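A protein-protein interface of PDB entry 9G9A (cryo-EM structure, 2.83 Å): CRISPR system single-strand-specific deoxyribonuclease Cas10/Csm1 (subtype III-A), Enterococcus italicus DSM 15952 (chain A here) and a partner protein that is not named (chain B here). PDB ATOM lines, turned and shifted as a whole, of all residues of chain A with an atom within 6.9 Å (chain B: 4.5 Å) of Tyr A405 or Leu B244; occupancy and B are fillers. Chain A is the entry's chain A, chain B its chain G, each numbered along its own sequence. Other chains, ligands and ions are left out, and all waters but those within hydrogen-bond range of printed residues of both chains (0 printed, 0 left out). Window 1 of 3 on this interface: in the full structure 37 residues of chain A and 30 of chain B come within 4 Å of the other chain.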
ATOM      1  N   LYS A 354      -2.177 -26.746  28.388  1.00  0.00           N
ATOM      2  CA  LYS A 354      -2.910 -25.504  28.173  1.00  0.00           C
ATOM      3  C   LYS A 354      -3.053 -24.727  29.474  1.00  0.00           C
ATOM      4  O   LYS A 354      -2.815 -23.514  29.516  1.00  0.00           O
ATOM      5  CB  LYS A 354      -4.286 -25.793  27.571  1.00  0.00           C
ATOM      6  CG  LYS A 354      -4.275 -26.072  26.082  1.00  0.00           C
ATOM      7  CD  LYS A 354      -5.682 -26.021  25.518  1.00  0.00           C
ATOM      8  CE  LYS A 354      -6.330 -24.675  25.799  1.00  0.00           C
ATOM      9  NZ  LYS A 354      -7.727 -24.604  25.293  1.00  0.00           N
ATOM     10  N   ILE A 358      -1.316 -21.093  30.178  1.00  0.00           N
ATOM     11  CA  ILE A 358      -2.155 -19.960  30.558  1.00  0.00           C
ATOM     12  C   ILE A 358      -1.685 -19.376  31.883  1.00  0.00           C
ATOM     13  O   ILE A 358      -1.604 -18.153  32.048  1.00  0.00           O
ATOM     14  CB  ILE A 358      -3.635 -20.378  30.616  1.00  0.00           C
ATOM     15  CG1 ILE A 358      -4.145 -20.729  29.218  1.00  0.00           C
ATOM     16  CG2 ILE A 358      -4.480 -19.276  31.229  1.00  0.00           C
ATOM     17  CD1 ILE A 358      -3.768 -19.722  28.170  1.00  0.00           C
ATOM     18  N   LYS A 362       0.273 -16.715  29.863  1.00  0.00           N
ATOM     19  CA  LYS A 362      -0.976 -16.126  29.358  1.00  0.00           C
ATOM     20  C   LYS A 362      -1.105 -16.507  27.882  1.00  0.00           C
ATOM     21  O   LYS A 362      -1.069 -17.703  27.561  1.00  0.00           O
ATOM     22  CB  LYS A 362      -0.990 -14.632  29.654  1.00  0.00           C
ATOM     23  CG  LYS A 362      -1.277 -14.275  31.101  1.00  0.00           C
ATOM     24  CD  LYS A 362      -2.767 -14.310  31.387  1.00  0.00           C
ATOM     25  CE  LYS A 362      -3.072 -13.764  32.772  1.00  0.00           C
ATOM     26  NZ  LYS A 362      -4.536 -13.672  33.024  1.00  0.00           N
ATOM     27  N   THR A 363      -1.253 -15.548  26.963  1.00  0.00           N
ATOM     28  CA  THR A 363      -1.404 -15.890  25.552  1.00  0.00           C
ATOM     29  C   THR A 363      -0.078 -15.846  24.805  1.00  0.00           C
ATOM     30  O   THR A 363      -0.049 -16.089  23.594  1.00  0.00           O
ATOM     31  CB  THR A 363      -2.406 -14.947  24.885  1.00  0.00           C
ATOM     32  OG1 THR A 363      -1.967 -13.592  25.044  1.00  0.00           O
ATOM     33  CG2 THR A 363      -3.778 -15.104  25.509  1.00  0.00           C
ATOM     34  N   ASP A 364       1.021 -15.533  25.495  1.00  0.00           N
ATOM     35  CA  ASP A 364       2.316 -15.417  24.830  1.00  0.00           C
ATOM     36  C   ASP A 364       2.730 -16.732  24.182  1.00  0.00           C
ATOM     37  O   ASP A 364       2.904 -16.814  22.961  1.00  0.00           O
ATOM     38  CB  ASP A 364       3.376 -14.950  25.830  1.00  0.00           C
ATOM     39  CG  ASP A 364       3.085 -13.571  26.380  1.00  0.00           C
ATOM     40  OD1 ASP A 364       2.592 -12.718  25.612  1.00  0.00           O
ATOM     41  OD2 ASP A 364       3.344 -13.340  27.580  1.00  0.00           O
ATOM     42  N   LEU A 365       2.893 -17.776  24.990  1.00  0.00           N
ATOM     43  CA  LEU A 365       3.288 -19.095  24.516  1.00  0.00           C
ATOM     44  C   LEU A 365       2.120 -20.058  24.661  1.00  0.00           C
ATOM     45  O   LEU A 365       1.383 -20.001  25.651  1.00  0.00           O
ATOM     46  CB  LEU A 365       4.497 -19.619  25.293  1.00  0.00           C
ATOM     47  CG  LEU A 365       5.848 -18.961  25.020  1.00  0.00           C
ATOM     48  CD1 LEU A 365       6.853 -19.379  26.067  1.00  0.00           C
ATOM     49  CD2 LEU A 365       6.346 -19.331  23.638  1.00  0.00           C
ATOM     50  N   SER A 366       1.956 -20.942  23.680  1.00  0.00           N
ATOM     51  CA  SER A 366       0.907 -21.950  23.727  1.00  0.00           C
ATOM     52  C   SER A 366       1.413 -23.226  23.072  1.00  0.00           C
ATOM     53  O   SER A 366       2.418 -23.223  22.362  1.00  0.00           O
ATOM     54  CB  SER A 366      -0.374 -21.467  23.036  1.00  0.00           C
ATOM     55  OG  SER A 366      -0.138 -21.168  21.673  1.00  0.00           O
ATOM     56  N   LYS A 400      -6.783 -26.753  15.381  1.00  0.00           N
ATOM     57  CA  LYS A 400      -6.672 -26.555  16.822  1.00  0.00           C
ATOM     58  C   LYS A 400      -6.019 -25.216  17.147  1.00  0.00           C
ATOM     59  O   LYS A 400      -6.421 -24.539  18.099  1.00  0.00           O
ATOM     60  CB  LYS A 400      -5.891 -27.703  17.456  1.00  0.00           C
ATOM     61  CG  LYS A 400      -6.729 -28.940  17.715  1.00  0.00           C
ATOM     62  CD  LYS A 400      -5.937 -29.982  18.475  1.00  0.00           C
ATOM     63  CE  LYS A 400      -6.831 -31.111  18.948  1.00  0.00           C
ATOM     64  NZ  LYS A 400      -7.842 -30.640  19.933  1.00  0.00           N
ATOM     65  N   LYS A 401      -5.006 -24.823  16.372  1.00  0.00           N
ATOM     66  CA  LYS A 401      -4.366 -23.528  16.582  1.00  0.00           C
ATOM     67  C   LYS A 401      -5.295 -22.361  16.276  1.00  0.00           C
ATOM     68  O   LYS A 401      -5.057 -21.252  16.766  1.00  0.00           O
ATOM     69  CB  LYS A 401      -3.100 -23.416  15.732  1.00  0.00           C
ATOM     70  CG  LYS A 401      -1.884 -24.086  16.345  1.00  0.00           C
ATOM     71  CD  LYS A 401      -1.580 -23.490  17.706  1.00  0.00           C
ATOM     72  CE  LYS A 401      -0.404 -24.177  18.376  1.00  0.00           C
ATOM     73  NZ  LYS A 401      -0.162 -23.618  19.732  1.00  0.00           N
ATOM     74  N   ALA A 402      -6.342 -22.579  15.477  1.00  0.00           N
ATOM     75  CA  ALA A 402      -7.295 -21.507  15.202  1.00  0.00           C
ATOM     76  C   ALA A 402      -8.130 -21.185  16.438  1.00  0.00           C
ATOM     77  O   ALA A 402      -8.095 -20.060  16.949  1.00  0.00           O
ATOM     78  CB  ALA A 402      -8.194 -21.894  14.026  1.00  0.00           C
ATOM     79  N   HIS A 403      -8.890 -22.163  16.930  1.00  0.00           N
ATOM     80  CA  HIS A 403      -9.681 -22.001  18.153  1.00  0.00           C
ATOM     81  C   HIS A 403      -8.820 -22.393  19.355  1.00  0.00           C
ATOM     82  O   HIS A 403      -8.963 -23.459  19.956  1.00  0.00           O
ATOM     83  CB  HIS A 403     -10.956 -22.831  18.075  1.00  0.00           C
ATOM     84  CG  HIS A 403     -11.992 -22.449  19.085  1.00  0.00           C
ATOM     85  ND1 HIS A 403     -11.829 -22.661  20.438  1.00  0.00           N
ATOM     86  CD2 HIS A 403     -13.210 -21.875  18.940  1.00  0.00           C
ATOM     87  CE1 HIS A 403     -12.898 -22.230  21.082  1.00  0.00           C
ATOM     88  NE2 HIS A 403     -13.751 -21.748  20.197  1.00  0.00           N
ATOM     89  N   LYS A 404      -7.902 -21.489  19.698  1.00  0.00           N
ATOM     90  CA  LYS A 404      -6.847 -21.826  20.648  1.00  0.00           C
ATOM     91  C   LYS A 404      -7.338 -21.835  22.091  1.00  0.00           C
ATOM     92  O   LYS A 404      -6.850 -22.632  22.900  1.00  0.00           O
ATOM     93  CB  LYS A 404      -5.678 -20.855  20.487  1.00  0.00           C
ATOM     94  CG  LYS A 404      -4.388 -21.321  21.129  1.00  0.00           C
ATOM     95  CD  LYS A 404      -3.238 -20.395  20.776  1.00  0.00           C
ATOM     96  CE  LYS A 404      -3.033 -20.317  19.275  1.00  0.00           C
ATOM     97  NZ  LYS A 404      -1.914 -19.403  18.917  1.00  0.00           N
ATOM     98  N   TYR A 405      -8.290 -20.972  22.440  1.00  0.00           N
ATOM     99  CA  TYR A 405      -8.731 -20.829  23.820  1.00  0.00           C
ATOM    100  C   TYR A 405     -10.238 -21.031  23.921  1.00  0.00           C
ATOM    101  O   TYR A 405     -10.977 -20.857  22.949  1.00  0.00           O
ATOM    102  CB  TYR A 405      -8.338 -19.459  24.385  1.00  0.00           C
ATOM    103  CG  TYR A 405      -6.874 -19.141  24.200  1.00  0.00           C
ATOM    104  CD1 TYR A 405      -5.907 -19.764  24.972  1.00  0.00           C
ATOM    105  CD2 TYR A 405      -6.457 -18.224  23.247  1.00  0.00           C
ATOM    106  CE1 TYR A 405      -4.566 -19.482  24.802  1.00  0.00           C
ATOM    107  CE2 TYR A 405      -5.119 -17.934  23.072  1.00  0.00           C
ATOM    108  CZ  TYR A 405      -4.177 -18.567  23.854  1.00  0.00           C
ATOM    109  OH  TYR A 405      -2.842 -18.285  23.685  1.00  0.00           O
ATOM    110  N   SER A 406     -10.687 -21.401  25.119  1.00  0.00           N
ATOM    111  CA  SER A 406     -12.078 -21.747  25.362  1.00  0.00           C
ATOM    112  C   SER A 406     -12.820 -20.579  26.010  1.00  0.00           C
ATOM    113  O   SER A 406     -12.274 -19.495  26.222  1.00  0.00           O
ATOM    114  CB  SER A 406     -12.172 -23.004  26.229  1.00  0.00           C
ATOM    115  OG  SER A 406     -11.596 -22.789  27.505  1.00  0.00           O
ATOM    116  N   LEU A 407     -14.095 -20.820  26.327  1.00  0.00           N
ATOM    117  CA  LEU A 407     -14.951 -19.769  26.872  1.00  0.00           C
ATOM    118  C   LEU A 407     -14.445 -19.285  28.227  1.00  0.00           C
ATOM    119  O   LEU A 407     -14.265 -18.079  28.442  1.00  0.00           O
ATOM    120  CB  LEU A 407     -16.385 -20.293  26.984  1.00  0.00           C
ATOM    121  CG  LEU A 407     -17.568 -19.334  27.149  1.00  0.00           C
ATOM    122  CD1 LEU A 407     -18.838 -20.037  26.717  1.00  0.00           C
ATOM    123  CD2 LEU A 407     -17.708 -18.849  28.581  1.00  0.00           C
ATOM    124  N   ASN A 408     -14.217 -20.217  29.156  1.00  0.00           N
ATOM    125  CA  ASN A 408     -13.807 -19.834  30.503  1.00  0.00           C
ATOM    126  C   ASN A 408     -12.443 -19.157  30.498  1.00  0.00           C
ATOM    127  O   ASN A 408     -12.217 -18.201  31.246  1.00  0.00           O
ATOM    128  CB  ASN A 408     -13.797 -21.057  31.420  1.00  0.00           C
ATOM    129  CG  ASN A 408     -15.193 -21.509  31.804  1.00  0.00           C
ATOM    130  OD1 ASN A 408     -16.113 -20.699  31.915  1.00  0.00           O
ATOM    131  ND2 ASN A 408     -15.357 -22.810  32.014  1.00  0.00           N
ATOM    132  N   GLU A 409     -11.519 -19.641  29.666  1.00  0.00           N
ATOM    133  CA  GLU A 409     -10.200 -19.022  29.596  1.00  0.00           C
ATOM    134  C   GLU A 409     -10.286 -17.601  29.052  1.00  0.00           C
ATOM    135  O   GLU A 409      -9.601 -16.698  29.544  1.00  0.00           O
ATOM    136  CB  GLU A 409      -9.267 -19.875  28.740  1.00  0.00           C
ATOM    137  CG  GLU A 409      -9.232 -21.335  29.150  1.00  0.00           C
ATOM    138  CD  GLU A 409      -8.274 -22.150  28.311  1.00  0.00           C
ATOM    139  OE1 GLU A 409      -7.159 -21.660  28.035  1.00  0.00           O
ATOM    140  OE2 GLU A 409      -8.639 -23.279  27.919  1.00  0.00           O
ATOM    141  N   ILE A 410     -11.127 -17.383  28.036  1.00  0.00           N
ATOM    142  CA  ILE A 410     -11.312 -16.037  27.499  1.00  0.00           C
ATOM    143  C   ILE A 410     -11.921 -15.120  28.553  1.00  0.00           C
ATOM    144  O   ILE A 410     -11.499 -13.968  28.715  1.00  0.00           O
ATOM    145  CB  ILE A 410     -12.165 -16.079  26.218  1.00  0.00           C
ATOM    146  CG1 ILE A 410     -11.369 -16.690  25.064  1.00  0.00           C
ATOM    147  CG2 ILE A 410     -12.638 -14.686  25.843  1.00  0.00           C
ATOM    148  CD1 ILE A 410     -12.130 -16.740  23.759  1.00  0.00           C
ATOM    149  N   PHE A 413      -9.342 -14.210  31.029  1.00  0.00           N
ATOM    150  CA  PHE A 413      -8.356 -13.284  30.481  1.00  0.00           C
ATOM    151  C   PHE A 413      -8.749 -11.836  30.751  1.00  0.00           C
ATOM    152  O   PHE A 413      -7.889 -10.993  31.029  1.00  0.00           O
ATOM    153  CB  PHE A 413      -8.187 -13.519  28.980  1.00  0.00           C
ATOM    154  CG  PHE A 413      -7.276 -14.664  28.644  1.00  0.00           C
ATOM    155  CD1 PHE A 413      -6.208 -14.981  29.464  1.00  0.00           C
ATOM    156  CD2 PHE A 413      -7.488 -15.422  27.505  1.00  0.00           C
ATOM    157  CE1 PHE A 413      -5.370 -16.030  29.153  1.00  0.00           C
ATOM    158  CE2 PHE A 413      -6.654 -16.472  27.191  1.00  0.00           C
ATOM    159  CZ  PHE A 413      -5.595 -16.776  28.017  1.00  0.00           C
ATOM    160  N   ASN A 414     -10.042 -11.534  30.681  1.00  0.00           N
ATOM    161  CA  ASN A 414     -10.541 -10.177  30.850  1.00  0.00           C
ATOM    162  C   ASN A 414     -10.950  -9.863  32.282  1.00  0.00           C
ATOM    163  O   ASN A 414     -11.517  -8.792  32.526  1.00  0.00           O
ATOM    164  CB  ASN A 414     -11.726  -9.934  29.910  1.00  0.00           C
ATOM    165  CG  ASN A 414     -11.331 -10.004  28.448  1.00  0.00           C
ATOM    166  OD1 ASN A 414     -10.215  -9.643  28.078  1.00  0.00           O
ATOM    167  ND2 ASN A 414     -12.248 -10.471  27.610  1.00  0.00           N
ATOM    168  N   MET B 227     -14.761  -7.986  21.141  1.00  0.00           N
ATOM    169  CA  MET B 227     -14.871  -9.026  22.153  1.00  0.00           C
ATOM    170  C   MET B 227     -16.290  -9.018  22.694  1.00  0.00           C
ATOM    171  O   MET B 227     -16.827  -7.955  23.016  1.00  0.00           O
ATOM    172  CB  MET B 227     -13.863  -8.812  23.287  1.00  0.00           C
ATOM    173  CG  MET B 227     -14.071  -9.729  24.479  1.00  0.00           C
ATOM    174  SD  MET B 227     -14.086 -11.472  24.029  1.00  0.00           S
ATOM    175  CE  MET B 227     -12.442 -11.659  23.351  1.00  0.00           C
ATOM    176  N   LEU B 237     -18.768 -18.338  20.456  1.00  0.00           N
ATOM    177  CA  LEU B 237     -17.450 -18.950  20.386  1.00  0.00           C
ATOM    178  C   LEU B 237     -17.475 -20.368  19.833  1.00  0.00           C
ATOM    179  O   LEU B 237     -16.417 -20.888  19.461  1.00  0.00           O
ATOM    180  CB  LEU B 237     -16.804 -18.951  21.774  1.00  0.00           C
ATOM    181  CG  LEU B 237     -15.282 -19.080  21.821  1.00  0.00           C
ATOM    182  CD1 LEU B 237     -14.627 -17.894  21.134  1.00  0.00           C
ATOM    183  CD2 LEU B 237     -14.807 -19.201  23.253  1.00  0.00           C
ATOM    184  N   TYR B 242     -10.518 -17.767  15.251  1.00  0.00           N
ATOM    185  CA  TYR B 242     -10.249 -16.404  15.681  1.00  0.00           C
ATOM    186  C   TYR B 242      -8.783 -16.265  16.068  1.00  0.00           C
ATOM    187  O   TYR B 242      -7.994 -17.210  15.972  1.00  0.00           O
ATOM    188  CB  TYR B 242     -11.146 -16.007  16.858  1.00  0.00           C
ATOM    189  CG  TYR B 242     -10.982 -16.889  18.073  1.00  0.00           C
ATOM    190  CD1 TYR B 242     -10.055 -16.583  19.057  1.00  0.00           C
ATOM    191  CD2 TYR B 242     -11.759 -18.025  18.237  1.00  0.00           C
ATOM    192  CE1 TYR B 242      -9.901 -17.384  20.165  1.00  0.00           C
ATOM    193  CE2 TYR B 242     -11.613 -18.830  19.342  1.00  0.00           C
ATOM    194  CZ  TYR B 242     -10.683 -18.504  20.302  1.00  0.00           C
ATOM    195  OH  TYR B 242     -10.532 -19.302  21.408  1.00  0.00           O
ATOM    196  N   LEU B 243      -8.430 -15.060  16.506  1.00  0.00           N
ATOM    197  CA  LEU B 243      -7.102 -14.751  17.014  1.00  0.00           C
ATOM    198  C   LEU B 243      -7.233 -13.748  18.150  1.00  0.00           C
ATOM    199  O   LEU B 243      -7.777 -12.656  17.957  1.00  0.00           O
ATOM    200  CB  LEU B 243      -6.205 -14.188  15.910  1.00  0.00           C
ATOM    201  CG  LEU B 243      -4.795 -13.761  16.325  1.00  0.00           C
ATOM    202  CD1 LEU B 243      -3.989 -14.949  16.823  1.00  0.00           C
ATOM    203  CD2 LEU B 243      -4.082 -13.071  15.174  1.00  0.00           C
ATOM    204  N   LEU B 244      -6.736 -14.117  19.328  1.00  0.00           N
ATOM    205  CA  LEU B 244      -6.793 -13.248  20.496  1.00  0.00           C
ATOM    206  C   LEU B 244      -5.588 -12.320  20.492  1.00  0.00           C
ATOM    207  O   LEU B 244      -4.441 -12.778  20.573  1.00  0.00           O
ATOM    208  CB  LEU B 244      -6.835 -14.062  21.789  1.00  0.00           C
ATOM    209  CG  LEU B 244      -8.220 -14.406  22.339  1.00  0.00           C
ATOM    210  CD1 LEU B 244      -8.104 -15.053  23.705  1.00  0.00           C
ATOM    211  CD2 LEU B 244      -9.086 -13.167  22.414  1.00  0.00           C
ATOM    212  N   LYS B 245      -5.846 -11.020  20.399  1.00  0.00           N
ATOM    213  CA  LYS B 245      -4.812  -9.998  20.425  1.00  0.00           C
ATOM    214  C   LYS B 245      -4.892  -9.281  21.765  1.00  0.00           C
ATOM    215  O   LYS B 245      -5.986  -8.912  22.214  1.00  0.00           O
ATOM    216  CB  LYS B 245      -4.980  -9.014  19.268  1.00  0.00           C
ATOM    217  CG  LYS B 245      -3.747  -8.164  18.999  1.00  0.00           C
ATOM    218  CD  LYS B 245      -3.879  -7.371  17.708  1.00  0.00           C
ATOM    219  CE  LYS B 245      -5.076  -6.438  17.751  1.00  0.00           C
ATOM    220  NZ  LYS B 245      -5.167  -5.606  16.521  1.00  0.00           N
ATOM    221  N   LYS B 246      -3.738  -9.114  22.405  1.00  0.00           N
ATOM    222  CA  LYS B 246      -3.680  -8.459  23.702  1.00  0.00           C
ATOM    223  C   LYS B 246      -3.534  -6.953  23.534  1.00  0.00           C
ATOM    224  O   LYS B 246      -2.508  -6.457  23.062  1.00  0.00           O
ATOM    225  CB  LYS B 246      -2.517  -9.013  24.523  1.00  0.00           C
ATOM    226  CG  LYS B 246      -2.457  -8.499  25.951  1.00  0.00           C
ATOM    227  CD  LYS B 246      -1.282  -9.097  26.709  1.00  0.00           C
ATOM    228  CE  LYS B 246       0.044  -8.744  26.048  1.00  0.00           C
ATOM    229  NZ  LYS B 246       1.204  -9.314  26.786  1.00  0.00           N
ATOM    230  N   TYR B 267      -8.190  -8.415  26.074  1.00  0.00           N
ATOM    231  CA  TYR B 267      -7.990  -9.399  25.019  1.00  0.00           C
ATOM    232  C   TYR B 267      -9.169  -9.341  24.064  1.00  0.00           C
ATOM    233  O   TYR B 267     -10.322  -9.486  24.487  1.00  0.00           O
ATOM    234  CB  TYR B 267      -7.825 -10.805  25.600  1.00  0.00           C
ATOM    235  CG  TYR B 267      -6.534 -10.984  26.364  1.00  0.00           C
ATOM    236  CD1 TYR B 267      -6.448 -10.659  27.707  1.00  0.00           C
ATOM    237  CD2 TYR B 267      -5.397 -11.469  25.735  1.00  0.00           C
ATOM    238  CE1 TYR B 267      -5.269 -10.817  28.406  1.00  0.00           C
ATOM    239  CE2 TYR B 267      -4.215 -11.630  26.426  1.00  0.00           C
ATOM    240  CZ  TYR B 267      -4.156 -11.302  27.761  1.00  0.00           C
ATOM    241  OH  TYR B 267      -2.979 -11.462  28.452  1.00  0.00           O
ATOM    242  N   ALA B 268      -8.887  -9.132  22.780  1.00  0.00           N
ATOM    243  CA  ALA B 268      -9.940  -8.932  21.797  1.00  0.00           C
ATOM    244  C   ALA B 268      -9.728  -9.837  20.595  1.00  0.00           C
ATOM    245  O   ALA B 268      -8.599 -10.201  20.259  1.00  0.00           O
ATOM    246  CB  ALA B 268     -10.003  -7.471  21.336  1.00  0.00           C
ATOM    247  N   PHE B 269     -10.829 -10.198  19.945  1.00  0.00           N
ATOM    248  CA  PHE B 269     -10.740 -10.970  18.715  1.00  0.00           C
ATOM    249  C   PHE B 269     -10.257 -10.072  17.582  1.00  0.00           C
ATOM    250  O   PHE B 269     -10.860  -9.032  17.299  1.00  0.00           O
ATOM    251  CB  PHE B 269     -12.096 -11.581  18.373  1.00  0.00           C
ATOM    252  CG  PHE B 269     -12.588 -12.571  19.390  1.00  0.00           C
ATOM    253  CD1 PHE B 269     -11.740 -13.536  19.904  1.00  0.00           C
ATOM    254  CD2 PHE B 269     -13.898 -12.532  19.835  1.00  0.00           C
ATOM    255  CE1 PHE B 269     -12.192 -14.447  20.837  1.00  0.00           C
ATOM    256  CE2 PHE B 269     -14.355 -13.440  20.769  1.00  0.00           C
ATOM    257  CZ  PHE B 269     -13.501 -14.398  21.270  1.00  0.00           C
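The backbone carbonyl oxygen of Lys A404 sits at hydrogen-bond distance from the side-chain amino group of Lys A354 (3.2 Å). A ring nitrogen (ND1) of His A403 sits close to the backbone carbonyl oxygen of Tyr A405. The side-chain hydroxyl (OG) of Ser A406 lies within hydrogen-bond range of the side-chain carboxylate (OE2) of Glu A409.
The side-chain amino group (NZ) of Lys B246 is in salt-bridge range of the side-chain carboxylate (OD1) of Asp A364 (3.9 Å). A ring nitrogen (NE2) of His A403 lies within hydrogen-bond range of the backbone carbonyl oxygen (O) of Leu B237 (2.9 Å). The backbone NH of Tyr A405 sits at hydrogen-bond distance from the side-chain hydroxyl of Tyr B242, at 3.0 Å. The side-chain amide oxygen (OD1) of Asn A414 is in hydrogen-bond range of the backbone NH (N) of Tyr B267, 3.1 Å away. O of Ala A402 sits close to O of Tyr B242 (3.0 Å).
Among the printed residues, pairs that only touch across the chains: Thr A363 with Tyr B267, His A403 with Tyr B242, Leu A407 with Leu B237, Phe A413 with Tyr B267, Tyr A405 with Leu B244, Ser A406 with Leu B237, Ile A410 with Leu B237, Ile A410 with Phe B269, Asn A414 with Met B227, Lys A404 with Tyr B242, Ile A410 with Tyr B242, Phe A413 with Leu B244, Ile A410 with Leu B244, Ile A410 with Met B227 and Lys A362 with Tyr B267.
Of the printed residues of chain B, Ala A402 touches Tyr B242 (3.0 Å). Tyr A405 touches two residues of chain B. Of the printed residues of chain B, Ser A406 touches Leu B237 (3.7 Å). Printed residues of chain A within 4 Å of Leu B237: His A403 (2.9 Å), Ser A406 (3.7 Å), Leu A407 (3.5 Å) and Ile A410 (3.7 Å). Of chain A, only Tyr A405 (3.6 Å), Ile A410 (3.9 Å) and Phe A413 (3.9 Å) come within 4 Å of Leu B244. The nearest printed residue of chain A that does not touch Tyr B242 is Ser A406 (4.3 Å).
Of the 10 printed residues of chain B, 7 touch a printed residue of chain A. Printed residues of chain B that touch a printed residue of chain A: Met B227, Leu B237, Tyr B242, Leu B244, Lys B246, Tyr B267 and Phe B269. Of the 20 printed residues of chain A, 12 touch a printed residue of chain B. Hydrophobic or aromatic side chains of chain A within 4 Å of the printed part of chain B: His A403, Tyr A405, Ile A410 and Phe A413.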
